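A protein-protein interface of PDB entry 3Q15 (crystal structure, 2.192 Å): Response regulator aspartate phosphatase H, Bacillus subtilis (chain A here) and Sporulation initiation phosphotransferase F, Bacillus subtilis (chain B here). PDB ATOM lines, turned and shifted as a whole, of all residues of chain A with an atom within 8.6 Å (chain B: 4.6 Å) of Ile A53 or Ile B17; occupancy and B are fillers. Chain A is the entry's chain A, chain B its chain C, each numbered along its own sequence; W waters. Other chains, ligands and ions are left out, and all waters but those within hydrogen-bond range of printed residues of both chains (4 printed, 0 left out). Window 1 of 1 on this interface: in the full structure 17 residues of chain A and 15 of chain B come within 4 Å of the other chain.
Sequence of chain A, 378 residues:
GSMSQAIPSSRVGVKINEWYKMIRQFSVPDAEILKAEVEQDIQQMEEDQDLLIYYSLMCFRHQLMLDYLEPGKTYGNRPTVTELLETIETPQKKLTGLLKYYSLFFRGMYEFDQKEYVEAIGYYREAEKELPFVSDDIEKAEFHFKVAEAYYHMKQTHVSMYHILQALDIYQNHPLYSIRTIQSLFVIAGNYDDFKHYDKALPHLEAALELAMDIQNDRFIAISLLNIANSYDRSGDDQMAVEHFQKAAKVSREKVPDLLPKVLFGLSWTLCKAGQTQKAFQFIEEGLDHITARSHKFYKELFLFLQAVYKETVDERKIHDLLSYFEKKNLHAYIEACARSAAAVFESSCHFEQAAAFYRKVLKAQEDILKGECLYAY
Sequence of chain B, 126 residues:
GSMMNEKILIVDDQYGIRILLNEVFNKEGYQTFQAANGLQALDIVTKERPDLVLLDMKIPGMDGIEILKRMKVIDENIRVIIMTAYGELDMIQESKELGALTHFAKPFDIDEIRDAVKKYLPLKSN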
ATOM      1  N   ILE A  16      14.464  16.340  -1.482  1.00  0.00           N
ATOM      2  CA  ILE A  16      15.081  17.657  -1.635  1.00  0.00           C
ATOM      3  C   ILE A  16      15.316  17.967  -3.117  1.00  0.00           C
ATOM      4  O   ILE A  16      15.126  19.098  -3.565  1.00  0.00           O
ATOM      5  CB  ILE A  16      16.412  17.757  -0.856  1.00  0.00           C
ATOM      6  CG1 ILE A  16      16.155  17.672   0.650  1.00  0.00           C
ATOM      7  CG2 ILE A  16      17.137  19.053  -1.192  1.00  0.00           C
ATOM      8  CD1 ILE A  16      17.397  17.823   1.500  1.00  0.00           C
ATOM      9  N   ILE A  42      13.517  14.902   8.310  1.00  0.00           N
ATOM     10  CA  ILE A  42      14.817  15.059   8.960  1.00  0.00           C
ATOM     11  C   ILE A  42      14.760  14.757  10.459  1.00  0.00           C
ATOM     12  O   ILE A  42      15.720  14.244  11.039  1.00  0.00           O
ATOM     13  CB  ILE A  42      15.401  16.465   8.721  1.00  0.00           C
ATOM     14  CG1 ILE A  42      15.773  16.632   7.247  1.00  0.00           C
ATOM     15  CG2 ILE A  42      16.611  16.696   9.603  1.00  0.00           C
ATOM     16  CD1 ILE A  42      16.408  17.956   6.920  1.00  0.00           C
ATOM     17  N   MET A  45      15.347  11.240  10.514  1.00  0.00           N
ATOM     18  CA  MET A  45      16.380  10.777   9.592  1.00  0.00           C
ATOM     19  C   MET A  45      17.620  10.265  10.316  1.00  0.00           C
ATOM     20  O   MET A  45      17.991  10.779  11.371  1.00  0.00           O
ATOM     21  CB  MET A  45      16.778  11.902   8.634  1.00  0.00           C
ATOM     22  CG  MET A  45      17.807  11.499   7.584  1.00  0.00           C
ATOM     23  SD  MET A  45      18.375  12.893   6.591  1.00  0.00           S
ATOM     24  CE  MET A  45      19.288  13.835   7.813  1.00  0.00           C
ATOM     25  N   ASP A  48      23.339  12.304   9.128  1.00  0.00           N
ATOM     26  CA  ASP A  48      24.079  12.580   7.901  1.00  0.00           C
ATOM     27  C   ASP A  48      24.261  14.085   7.745  1.00  0.00           C
ATOM     28  O   ASP A  48      23.419  14.764   7.154  1.00  0.00           O
ATOM     29  CB  ASP A  48      23.348  12.016   6.679  1.00  0.00           C
ATOM     30  CG  ASP A  48      24.180  12.100   5.406  1.00  0.00           C
ATOM     31  OD1 ASP A  48      25.119  12.922   5.353  1.00  0.00           O
ATOM     32  OD2 ASP A  48      23.898  11.341   4.456  1.00  0.00           O
ATOM     33  N   GLN A  49      25.362  14.604   8.274  1.00  0.00           N
ATOM     34  CA  GLN A  49      25.602  16.040   8.236  1.00  0.00           C
ATOM     35  C   GLN A  49      25.705  16.584   6.809  1.00  0.00           C
ATOM     36  O   GLN A  49      25.505  17.776   6.582  1.00  0.00           O
ATOM     37  CB  GLN A  49      26.846  16.410   9.055  1.00  0.00           C
ATOM     38  CG  GLN A  49      28.128  15.740   8.602  1.00  0.00           C
ATOM     39  CD  GLN A  49      29.317  16.097   9.482  1.00  0.00           C
ATOM     40  OE1 GLN A  49      30.344  15.420   9.456  1.00  0.00           O
ATOM     41  NE2 GLN A  49      29.182  17.165  10.262  1.00  0.00           N
ATOM     42  N   ASP A  50      26.013  15.711   5.853  1.00  0.00           N
ATOM     43  CA  ASP A  50      26.100  16.122   4.455  1.00  0.00           C
ATOM     44  C   ASP A  50      24.713  16.447   3.916  1.00  0.00           C
ATOM     45  O   ASP A  50      24.543  17.381   3.131  1.00  0.00           O
ATOM     46  CB  ASP A  50      26.734  15.026   3.597  1.00  0.00           C
ATOM     47  CG  ASP A  50      28.165  14.731   3.987  1.00  0.00           C
ATOM     48  OD1 ASP A  50      28.879  15.665   4.410  1.00  0.00           O
ATOM     49  OD2 ASP A  50      28.575  13.557   3.865  1.00  0.00           O
ATOM     50  N   LEU A  51      23.726  15.661   4.339  1.00  0.00           N
ATOM     51  CA  LEU A  51      22.343  15.886   3.950  1.00  0.00           C
ATOM     52  C   LEU A  51      21.867  17.223   4.505  1.00  0.00           C
ATOM     53  O   LEU A  51      21.233  18.007   3.797  1.00  0.00           O
ATOM     54  CB  LEU A  51      21.454  14.745   4.455  1.00  0.00           C
ATOM     55  CG  LEU A  51      19.990  14.707   3.996  1.00  0.00           C
ATOM     56  CD1 LEU A  51      19.162  15.783   4.686  1.00  0.00           C
ATOM     57  CD2 LEU A  51      19.893  14.829   2.480  1.00  0.00           C
ATOM     58  N   LEU A  52      22.187  17.479   5.770  1.00  0.00           N
ATOM     59  CA  LEU A  52      21.784  18.718   6.434  1.00  0.00           C
ATOM     60  C   LEU A  52      22.365  19.955   5.753  1.00  0.00           C
ATOM     61  O   LEU A  52      21.728  21.005   5.715  1.00  0.00           O
ATOM     62  CB  LEU A  52      22.192  18.703   7.907  1.00  0.00           C
ATOM     63  CG  LEU A  52      21.646  17.565   8.767  1.00  0.00           C
ATOM     64  CD1 LEU A  52      22.097  17.735  10.209  1.00  0.00           C
ATOM     65  CD2 LEU A  52      20.131  17.505   8.683  1.00  0.00           C
ATOM     66  N   ILE A  53      23.582  19.831   5.231  1.00  0.00           N
ATOM     67  CA  ILE A  53      24.200  20.913   4.478  1.00  0.00           C
ATOM     68  C   ILE A  53      23.422  21.156   3.195  1.00  0.00           C
ATOM     69  O   ILE A  53      23.121  22.294   2.849  1.00  0.00           O
ATOM     70  CB  ILE A  53      25.662  20.592   4.118  1.00  0.00           C
ATOM     71  CG1 ILE A  53      26.517  20.508   5.384  1.00  0.00           C
ATOM     72  CG2 ILE A  53      26.217  21.646   3.170  1.00  0.00           C
ATOM     73  CD1 ILE A  53      27.977  20.273   5.100  1.00  0.00           C
ATOM     74  N   TYR A  54      23.093  20.073   2.498  1.00  0.00           N
ATOM     75  CA  TYR A  54      22.304  20.152   1.272  1.00  0.00           C
ATOM     76  C   TYR A  54      20.953  20.801   1.566  1.00  0.00           C
ATOM     77  O   TYR A  54      20.454  21.613   0.784  1.00  0.00           O
ATOM     78  CB  TYR A  54      22.118  18.750   0.683  1.00  0.00           C
ATOM     79  CG  TYR A  54      21.372  18.700  -0.632  1.00  0.00           C
ATOM     80  CD1 TYR A  54      21.382  19.775  -1.512  1.00  0.00           C
ATOM     81  CD2 TYR A  54      20.648  17.568  -0.992  1.00  0.00           C
ATOM     82  CE1 TYR A  54      20.697  19.720  -2.715  1.00  0.00           C
ATOM     83  CE2 TYR A  54      19.962  17.506  -2.186  1.00  0.00           C
ATOM     84  CZ  TYR A  54      19.988  18.584  -3.045  1.00  0.00           C
ATOM     85  OH  TYR A  54      19.299  18.520  -4.238  1.00  0.00           O
ATOM     86  N   TYR A  55      20.372  20.447   2.709  1.00  0.00           N
ATOM     87  CA  TYR A  55      19.112  21.037   3.147  1.00  0.00           C
ATOM     88  C   TYR A  55      19.227  22.547   3.372  1.00  0.00           C
ATOM     89  O   TYR A  55      18.373  23.313   2.923  1.00  0.00           O
ATOM     90  CB  TYR A  55      18.611  20.353   4.423  1.00  0.00           C
ATOM     91  CG  TYR A  55      17.587  21.167   5.183  1.00  0.00           C
ATOM     92  CD1 TYR A  55      16.249  21.160   4.813  1.00  0.00           C
ATOM     93  CD2 TYR A  55      17.962  21.947   6.268  1.00  0.00           C
ATOM     94  CE1 TYR A  55      15.312  21.908   5.506  1.00  0.00           C
ATOM     95  CE2 TYR A  55      17.032  22.698   6.966  1.00  0.00           C
ATOM     96  CZ  TYR A  55      15.709  22.674   6.580  1.00  0.00           C
ATOM     97  OH  TYR A  55      14.785  23.421   7.273  1.00  0.00           O
ATOM     98  N   SER A  56      20.277  22.963   4.077  1.00  0.00           N
ATOM     99  CA  SER A  56      20.485  24.375   4.391  1.00  0.00           C
ATOM    100  C   SER A  56      20.760  25.211   3.146  1.00  0.00           C
ATOM    101  O   SER A  56      20.277  26.337   3.026  1.00  0.00           O
ATOM    102  CB  SER A  56      21.618  24.551   5.407  1.00  0.00           C
ATOM    103  OG  SER A  56      21.240  24.041   6.673  1.00  0.00           O
ATOM    104  N   LEU A  57      21.540  24.663   2.222  1.00  0.00           N
ATOM    105  CA  LEU A  57      21.770  25.332   0.951  1.00  0.00           C
ATOM    106  C   LEU A  57      20.456  25.469   0.177  1.00  0.00           C
ATOM    107  O   LEU A  57      20.181  26.511  -0.422  1.00  0.00           O
ATOM    108  CB  LEU A  57      22.804  24.571   0.121  1.00  0.00           C
ATOM    109  CG  LEU A  57      24.219  24.470   0.700  1.00  0.00           C
ATOM    110  CD1 LEU A  57      25.092  23.580  -0.178  1.00  0.00           C
ATOM    111  CD2 LEU A  57      24.847  25.854   0.870  1.00  0.00           C
ATOM    112  N   MET A  58      19.641  24.417   0.195  1.00  0.00           N
ATOM    113  CA  MET A  58      18.356  24.469  -0.491  1.00  0.00           C
ATOM    114  C   MET A  58      17.439  25.510   0.150  1.00  0.00           C
ATOM    115  O   MET A  58      16.711  26.211  -0.548  1.00  0.00           O
ATOM    116  CB  MET A  58      17.676  23.099  -0.526  1.00  0.00           C
ATOM    117  CG  MET A  58      16.496  23.040  -1.482  1.00  0.00           C
ATOM    118  SD  MET A  58      16.968  23.396  -3.187  1.00  0.00           S
ATOM    119  CE  MET A  58      18.168  22.098  -3.482  1.00  0.00           C
ATOM    120  N   CYS A  59      17.485  25.615   1.475  1.00  0.00           N
ATOM    121  CA  CYS A  59      16.728  26.644   2.183  1.00  0.00           C
ATOM    122  C   CYS A  59      17.100  28.033   1.669  1.00  0.00           C
ATOM    123  O   CYS A  59      16.244  28.911   1.547  1.00  0.00           O
ATOM    124  CB  CYS A  59      16.974  26.566   3.694  1.00  0.00           C
ATOM    125  SG  CYS A  59      16.110  25.219   4.538  1.00  0.00           S
ATOM    126  N   PHE A  60      18.381  28.219   1.371  1.00  0.00           N
ATOM    127  CA  PHE A  60      18.882  29.500   0.889  1.00  0.00           C
ATOM    128  C   PHE A  60      18.422  29.729  -0.547  1.00  0.00           C
ATOM    129  O   PHE A  60      17.974  30.819  -0.905  1.00  0.00           O
ATOM    130  CB  PHE A  60      20.412  29.536   0.980  1.00  0.00           C
ATOM    131  CG  PHE A  60      21.021  30.857   0.588  1.00  0.00           C
ATOM    132  CD1 PHE A  60      20.976  31.940   1.451  1.00  0.00           C
ATOM    133  CD2 PHE A  60      21.659  31.006  -0.634  1.00  0.00           C
ATOM    134  CE1 PHE A  60      21.540  33.154   1.095  1.00  0.00           C
ATOM    135  CE2 PHE A  60      22.225  32.218  -0.995  1.00  0.00           C
ATOM    136  CZ  PHE A  60      22.167  33.293  -0.129  1.00  0.00           C
ATOM    137  N   LEU A  95      26.962  28.229  -5.508  1.00  0.00           N
ATOM    138  CA  LEU A  95      25.777  27.638  -4.899  1.00  0.00           C
ATOM    139  C   LEU A  95      25.104  26.677  -5.869  1.00  0.00           C
ATOM    140  O   LEU A  95      24.778  25.541  -5.521  1.00  0.00           O
ATOM    141  CB  LEU A  95      24.784  28.730  -4.500  1.00  0.00           C
ATOM    142  CG  LEU A  95      23.405  28.218  -4.082  1.00  0.00           C
ATOM    143  CD1 LEU A  95      23.508  27.369  -2.820  1.00  0.00           C
ATOM    144  CD2 LEU A  95      22.429  29.368  -3.887  1.00  0.00           C
ATOM    145  N   LEU A  98      27.208  23.539  -6.370  1.00  0.00           N
ATOM    146  CA  LEU A  98      27.186  22.637  -5.224  1.00  0.00           C
ATOM    147  C   LEU A  98      25.855  21.899  -5.126  1.00  0.00           C
ATOM    148  O   LEU A  98      25.824  20.692  -4.878  1.00  0.00           O
ATOM    149  CB  LEU A  98      27.472  23.402  -3.932  1.00  0.00           C
ATOM    150  CG  LEU A  98      27.747  22.548  -2.692  1.00  0.00           C
ATOM    151  CD1 LEU A  98      28.662  21.375  -3.028  1.00  0.00           C
ATOM    152  CD2 LEU A  98      28.346  23.404  -1.585  1.00  0.00           C
ATOM    153  N   LEU A  99      24.758  22.627  -5.327  1.00  0.00           N
ATOM    154  CA  LEU A  99      23.431  22.017  -5.319  1.00  0.00           C
ATOM    155  C   LEU A  99      23.346  20.905  -6.353  1.00  0.00           C
ATOM    156  O   LEU A  99      22.846  19.817  -6.071  1.00  0.00           O
ATOM    157  CB  LEU A  99      22.343  23.058  -5.598  1.00  0.00           C
ATOM    158  CG  LEU A  99      22.102  24.118  -4.527  1.00  0.00           C
ATOM    159  CD1 LEU A  99      20.986  25.050  -4.972  1.00  0.00           C
ATOM    160  CD2 LEU A  99      21.767  23.468  -3.195  1.00  0.00           C
ATOM    161  N   TYR A 102      25.171  17.822  -5.113  1.00  0.00           N
ATOM    162  CA  TYR A 102      24.418  17.100  -4.098  1.00  0.00           C
ATOM    163  C   TYR A 102      23.230  16.338  -4.683  1.00  0.00           C
ATOM    164  O   TYR A 102      22.995  15.183  -4.328  1.00  0.00           O
ATOM    165  CB  TYR A 102      23.947  18.060  -3.007  1.00  0.00           C
ATOM    166  CG  TYR A 102      25.000  18.349  -1.957  1.00  0.00           C
ATOM    167  CD1 TYR A 102      25.161  19.630  -1.444  1.00  0.00           C
ATOM    168  CD2 TYR A 102      25.822  17.340  -1.472  1.00  0.00           C
ATOM    169  CE1 TYR A 102      26.115  19.901  -0.484  1.00  0.00           C
ATOM    170  CE2 TYR A 102      26.782  17.600  -0.508  1.00  0.00           C
ATOM    171  CZ  TYR A 102      26.922  18.887  -0.019  1.00  0.00           C
ATOM    172  OH  TYR A 102      27.866  19.169   0.937  1.00  0.00           O
ATOM    173  N   PHE A 106      23.216  12.376  -3.916  1.00  0.00           N
ATOM    174  CA  PHE A 106      22.177  11.714  -3.139  1.00  0.00           C
ATOM    175  C   PHE A 106      21.236  10.873  -3.994  1.00  0.00           C
ATOM    176  O   PHE A 106      20.651   9.912  -3.506  1.00  0.00           O
ATOM    177  CB  PHE A 106      21.394  12.726  -2.311  1.00  0.00           C
ATOM    178  CG  PHE A 106      22.141  13.205  -1.111  1.00  0.00           C
ATOM    179  CD1 PHE A 106      22.352  12.360  -0.035  1.00  0.00           C
ATOM    180  CD2 PHE A 106      22.653  14.489  -1.062  1.00  0.00           C
ATOM    181  CE1 PHE A 106      23.056  12.791   1.077  1.00  0.00           C
ATOM    182  CE2 PHE A 106      23.353  14.926   0.046  1.00  0.00           C
ATOM    183  CZ  PHE A 106      23.556  14.077   1.117  1.00  0.00           C
ATOM    184  N   GLU A 139      36.478  17.794   0.136  1.00  0.00           N
ATOM    185  CA  GLU A 139      35.193  17.493  -0.480  1.00  0.00           C
ATOM    186  C   GLU A 139      35.388  16.404  -1.531  1.00  0.00           C
ATOM    187  O   GLU A 139      34.609  15.451  -1.603  1.00  0.00           O
ATOM    188  CB  GLU A 139      34.582  18.748  -1.110  1.00  0.00           C
ATOM    189  CG  GLU A 139      33.095  18.630  -1.418  1.00  0.00           C
ATOM    190  CD  GLU A 139      32.262  18.382  -0.172  1.00  0.00           C
ATOM    191  OE1 GLU A 139      32.567  18.983   0.880  1.00  0.00           O
ATOM    192  OE2 GLU A 139      31.307  17.579  -0.240  1.00  0.00           O
ATOM    193  N   ASP B  12      34.721  26.373   9.484  1.00  0.00           N
ATOM    194  CA  ASP B  12      34.028  25.109   9.258  1.00  0.00           C
ATOM    195  C   ASP B  12      34.778  24.250   8.244  1.00  0.00           C
ATOM    196  O   ASP B  12      35.275  24.754   7.234  1.00  0.00           O
ATOM    197  CB  ASP B  12      32.592  25.353   8.785  1.00  0.00           C
ATOM    198  CG  ASP B  12      31.719  24.119   8.914  1.00  0.00           C
ATOM    199  OD1 ASP B  12      31.834  23.207   8.065  1.00  0.00           O
ATOM    200  OD2 ASP B  12      30.916  24.064   9.867  1.00  0.00           O
ATOM    201  N   GLN B  14      33.617  22.007   6.299  1.00  0.00           N
ATOM    202  CA  GLN B  14      32.826  21.621   5.137  1.00  0.00           C
ATOM    203  C   GLN B  14      32.556  22.782   4.180  1.00  0.00           C
ATOM    204  O   GLN B  14      31.992  23.810   4.561  1.00  0.00           O
ATOM    205  CB  GLN B  14      31.530  20.925   5.566  1.00  0.00           C
ATOM    206  CG  GLN B  14      31.774  19.625   6.334  1.00  0.00           C
ATOM    207  CD  GLN B  14      30.524  18.776   6.488  1.00  0.00           C
ATOM    208  OE1 GLN B  14      29.770  18.929   7.449  1.00  0.00           O
ATOM    209  NE2 GLN B  14      30.303  17.869   5.541  1.00  0.00           N
ATOM    210  N   TYR B  15      32.978  22.593   2.935  1.00  0.00           N
ATOM    211  CA  TYR B  15      32.843  23.588   1.881  1.00  0.00           C
ATOM    212  C   TYR B  15      31.440  24.187   1.818  1.00  0.00           C
ATOM    213  O   TYR B  15      31.279  25.396   1.656  1.00  0.00           O
ATOM    214  CB  TYR B  15      33.219  22.955   0.537  1.00  0.00           C
ATOM    215  CG  TYR B  15      33.064  23.857  -0.667  1.00  0.00           C
ATOM    216  CD1 TYR B  15      33.889  24.958  -0.847  1.00  0.00           C
ATOM    217  CD2 TYR B  15      32.108  23.589  -1.639  1.00  0.00           C
ATOM    218  CE1 TYR B  15      33.755  25.780  -1.951  1.00  0.00           C
ATOM    219  CE2 TYR B  15      31.968  24.402  -2.747  1.00  0.00           C
ATOM    220  CZ  TYR B  15      32.793  25.494  -2.898  1.00  0.00           C
ATOM    221  OH  TYR B  15      32.655  26.305  -4.000  1.00  0.00           O
ATOM    222  N   GLY B  16      30.428  23.334   1.955  1.00  0.00           N
ATOM    223  CA  GLY B  16      29.040  23.757   1.868  1.00  0.00           C
ATOM    224  C   GLY B  16      28.655  24.848   2.851  1.00  0.00           C
ATOM    225  O   GLY B  16      28.062  25.855   2.465  1.00  0.00           O
ATOM    226  N   ILE B  17      28.984  24.644   4.123  1.00  0.00           N
ATOM    227  CA  ILE B  17      28.668  25.615   5.164  1.00  0.00           C
ATOM    228  C   ILE B  17      29.379  26.945   4.913  1.00  0.00           C
ATOM    229  O   ILE B  17      28.787  28.015   5.062  1.00  0.00           O
ATOM    230  CB  ILE B  17      29.057  25.088   6.561  1.00  0.00           C
ATOM    231  CG1 ILE B  17      28.317  23.781   6.868  1.00  0.00           C
ATOM    232  CG2 ILE B  17      28.770  26.135   7.628  1.00  0.00           C
ATOM    233  CD1 ILE B  17      26.812  23.924   6.929  1.00  0.00           C
ATOM    234  N   ARG B  18      30.649  26.871   4.528  1.00  0.00           N
ATOM    235  CA  ARG B  18      31.435  28.071   4.258  1.00  0.00           C
ATOM    236  C   ARG B  18      30.862  28.897   3.102  1.00  0.00           C
ATOM    237  O   ARG B  18      30.758  30.120   3.195  1.00  0.00           O
ATOM    238  CB  ARG B  18      32.905  27.717   4.014  1.00  0.00           C
ATOM    239  CG  ARG B  18      33.694  27.508   5.299  1.00  0.00           C
ATOM    240  CD  ARG B  18      35.180  27.299   5.045  1.00  0.00           C
ATOM    241  NE  ARG B  18      35.484  25.923   4.667  1.00  0.00           N
ATOM    242  CZ  ARG B  18      35.933  25.555   3.473  1.00  0.00           C
ATOM    243  NH1 ARG B  18      36.144  26.465   2.532  1.00  0.00           N
ATOM    244  NH2 ARG B  18      36.179  24.276   3.223  1.00  0.00           N
ATOM    245  N   ILE B  19      30.493  28.227   2.017  1.00  0.00           N
ATOM    246  CA  ILE B  19      29.844  28.901   0.902  1.00  0.00           C
ATOM    247  C   ILE B  19      28.570  29.599   1.368  1.00  0.00           C
ATOM    248  O   ILE B  19      28.328  30.759   1.034  1.00  0.00           O
ATOM    249  CB  ILE B  19      29.499  27.911  -0.227  1.00  0.00           C
ATOM    250  CG1 ILE B  19      30.773  27.428  -0.918  1.00  0.00           C
ATOM    251  CG2 ILE B  19      28.566  28.552  -1.243  1.00  0.00           C
ATOM    252  CD1 ILE B  19      31.567  28.532  -1.573  1.00  0.00           C
ATOM    253  N   LEU B  20      27.767  28.889   2.153  1.00  0.00           N
ATOM    254  CA  LEU B  20      26.483  29.411   2.618  1.00  0.00           C
ATOM    255  C   LEU B  20      26.644  30.687   3.438  1.00  0.00           C
ATOM    256  O   LEU B  20      26.163  31.751   3.047  1.00  0.00           O
ATOM    257  CB  LEU B  20      25.739  28.355   3.438  1.00  0.00           C
ATOM    258  CG  LEU B  20      24.391  28.787   4.026  1.00  0.00           C
ATOM    259  CD1 LEU B  20      23.395  29.117   2.919  1.00  0.00           C
ATOM    260  CD2 LEU B  20      23.840  27.713   4.950  1.00  0.00           C
ATOM    261  N   LEU B  21      27.323  30.571   4.575  1.00  0.00           N
ATOM    262  CA  LEU B  21      27.510  31.705   5.476  1.00  0.00           C
ATOM    263  C   LEU B  21      28.216  32.873   4.793  1.00  0.00           C
ATOM    264  O   LEU B  21      27.951  34.032   5.105  1.00  0.00           O
ATOM    265  CB  LEU B  21      28.275  31.276   6.732  1.00  0.00           C
ATOM    266  CG  LEU B  21      27.558  30.231   7.594  1.00  0.00           C
ATOM    267  CD1 LEU B  21      28.391  29.857   8.808  1.00  0.00           C
ATOM    268  CD2 LEU B  21      26.196  30.746   8.019  1.00  0.00           C
ATOM    269  N   MET B  83      28.631  26.486  16.494  1.00  0.00           N
ATOM    270  CA  MET B  83      27.583  25.767  15.787  1.00  0.00           C
ATOM    271  C   MET B  83      27.952  24.292  15.725  1.00  0.00           C
ATOM    272  O   MET B  83      29.122  23.945  15.562  1.00  0.00           O
ATOM    273  CB  MET B  83      27.399  26.342  14.384  1.00  0.00           C
ATOM    274  CG  MET B  83      28.692  26.484  13.607  1.00  0.00           C
ATOM    275  SD  MET B  83      28.503  27.453  12.099  1.00  0.00           S
ATOM    276  CE  MET B  83      30.173  27.365  11.456  1.00  0.00           C
ATOM    277  N   LYS B 106      22.770  22.636  13.897  1.00  0.00           N
ATOM    278  CA  LYS B 106      22.569  22.396  12.474  1.00  0.00           C
ATOM    279  C   LYS B 106      21.421  21.409  12.268  1.00  0.00           C
ATOM    280  O   LYS B 106      21.289  20.449  13.026  1.00  0.00           O
ATOM    281  CB  LYS B 106      23.850  21.847  11.844  1.00  0.00           C
ATOM    282  CG  LYS B 106      25.042  22.790  11.922  1.00  0.00           C
ATOM    283  CD  LYS B 106      26.264  22.181  11.255  1.00  0.00           C
ATOM    284  CE  LYS B 106      27.441  23.138  11.259  1.00  0.00           C
ATOM    285  NZ  LYS B 106      28.634  22.527  10.612  1.00  0.00           N
ATOM    286  N   PHE B 108      20.938  25.108  11.019  1.00  0.00           N
ATOM    287  CA  PHE B 108      20.529  26.356  11.644  1.00  0.00           C
ATOM    288  C   PHE B 108      19.641  27.170  10.718  1.00  0.00           C
ATOM    289  O   PHE B 108      19.771  27.102   9.497  1.00  0.00           O
ATOM    290  CB  PHE B 108      21.746  27.180  12.076  1.00  0.00           C
ATOM    291  CG  PHE B 108      22.796  27.329  11.008  1.00  0.00           C
ATOM    292  CD1 PHE B 108      22.573  28.132   9.901  1.00  0.00           C
ATOM    293  CD2 PHE B 108      24.013  26.676  11.120  1.00  0.00           C
ATOM    294  CE1 PHE B 108      23.540  28.272   8.921  1.00  0.00           C
ATOM    295  CE2 PHE B 108      24.984  26.813  10.144  1.00  0.00           C
ATOM    296  CZ  PHE B 108      24.747  27.611   9.043  1.00  0.00           C
HETATM  297  O   HOH W   1      30.171  20.612   1.747  1.00  0.00           O
HETATM  298  O   HOH W   2      22.981  24.409   9.162  1.00  0.00           O
HETATM  299  O   HOH W   3      30.435  24.805  -6.016  1.00  0.00           O
HETATM  300  O   HOH W   4      34.334  20.216   2.464  1.00  0.00           O
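Water W4 bridges the side-chain carboxylate of Glu A139 (2.7 Å) and the backbone NH of Tyr B15 (2.8 Å).
Water W1 lies within hydrogen-bond range of the backbone NH of Gly B16 (2.7 Å), the side-chain hydroxyl of Tyr A102 (2.8 Å) and the side-chain carboxylate of Glu A139 (3.0 Å).
Water W2 bridges the backbone NH of Phe B108 (2.8 Å) and the side-chain hydroxyl of Ser A56 (3.1 Å).
Water W3 bridges OH of Tyr B15 (3.4 Å) and N of Leu A98 (3.5 Å).
Hydrophobic or aromatic side chains of chain B that line the printed part of chain A: Tyr B15, Ile B17 and Leu B20.
Along chain B the printed residues that touch a printed residue of chain A span positions 14 to 106.
Among the printed residues, no Asp or Glu carboxylate lies within 4 Å of a Lys or Arg side-chain nitrogen of the other chain.
Among the printed residues, merely in contact across the chains: Leu A52 with Lys B106 (3.99 Å), Ile A53 with Gln B14 (3.2 Å), Ile A53 with Gly B16 (3.8 Å), Ile A53 with Ile B17 (3.8 Å), Ser A56 with Leu B20 (3.9 Å), Leu A57 with Gly B16 (3.6 Å), Leu A57 with Leu B20 (3.7 Å), Phe A60 with Leu B20 (3.6 Å), Leu A98 with Tyr B15 (3.8 Å) and Leu A98 with Gly B16 (3.5 Å).
The side-chain carboxylate (OD1) of Asp A50 sits at hydrogen-bond distance from the side-chain amide nitrogen (NE2) of Gln B14, 2.9 Å away.
NE2 of Gln A49 is in hydrogen-bond range of OE1 of Gln B14, at 3.4 Å.
Printed residues of chain B within 4 Å of Asp A50: Gln B14 (2.9 Å).
Of chain B, only Gln B14 (3.2 Å), Gly B16 (3.8 Å) and Ile B17 (3.8 Å) come within 4 Å of Ile A53.
Of the printed residues of chain B, Leu A57 touches Gly B16 (3.6 Å) and Leu B20 (3.7 Å).
Leu A95 touches none of the printed residues of chain B.
Ile B17 touches just one residue of chain A: Ile A53 (3.8 Å).
Met B83 touches none of the printed residues of chain A.
OD1 of Asp B12 lies within hydrogen-bond range of N of Gln B14, 2.8 Å away.
NZ of Lys B106 lies within salt-bridge range of OD2 of Asp B12 (2.9 Å).
OD1 of Asp A48 sits at hydrogen-bond distance from N of Asp A50, 3.0 Å away.
The backbone carbonyl oxygen (O) of Leu A52 sits at hydrogen-bond distance from the side-chain hydroxyl (OG) of Ser A56.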
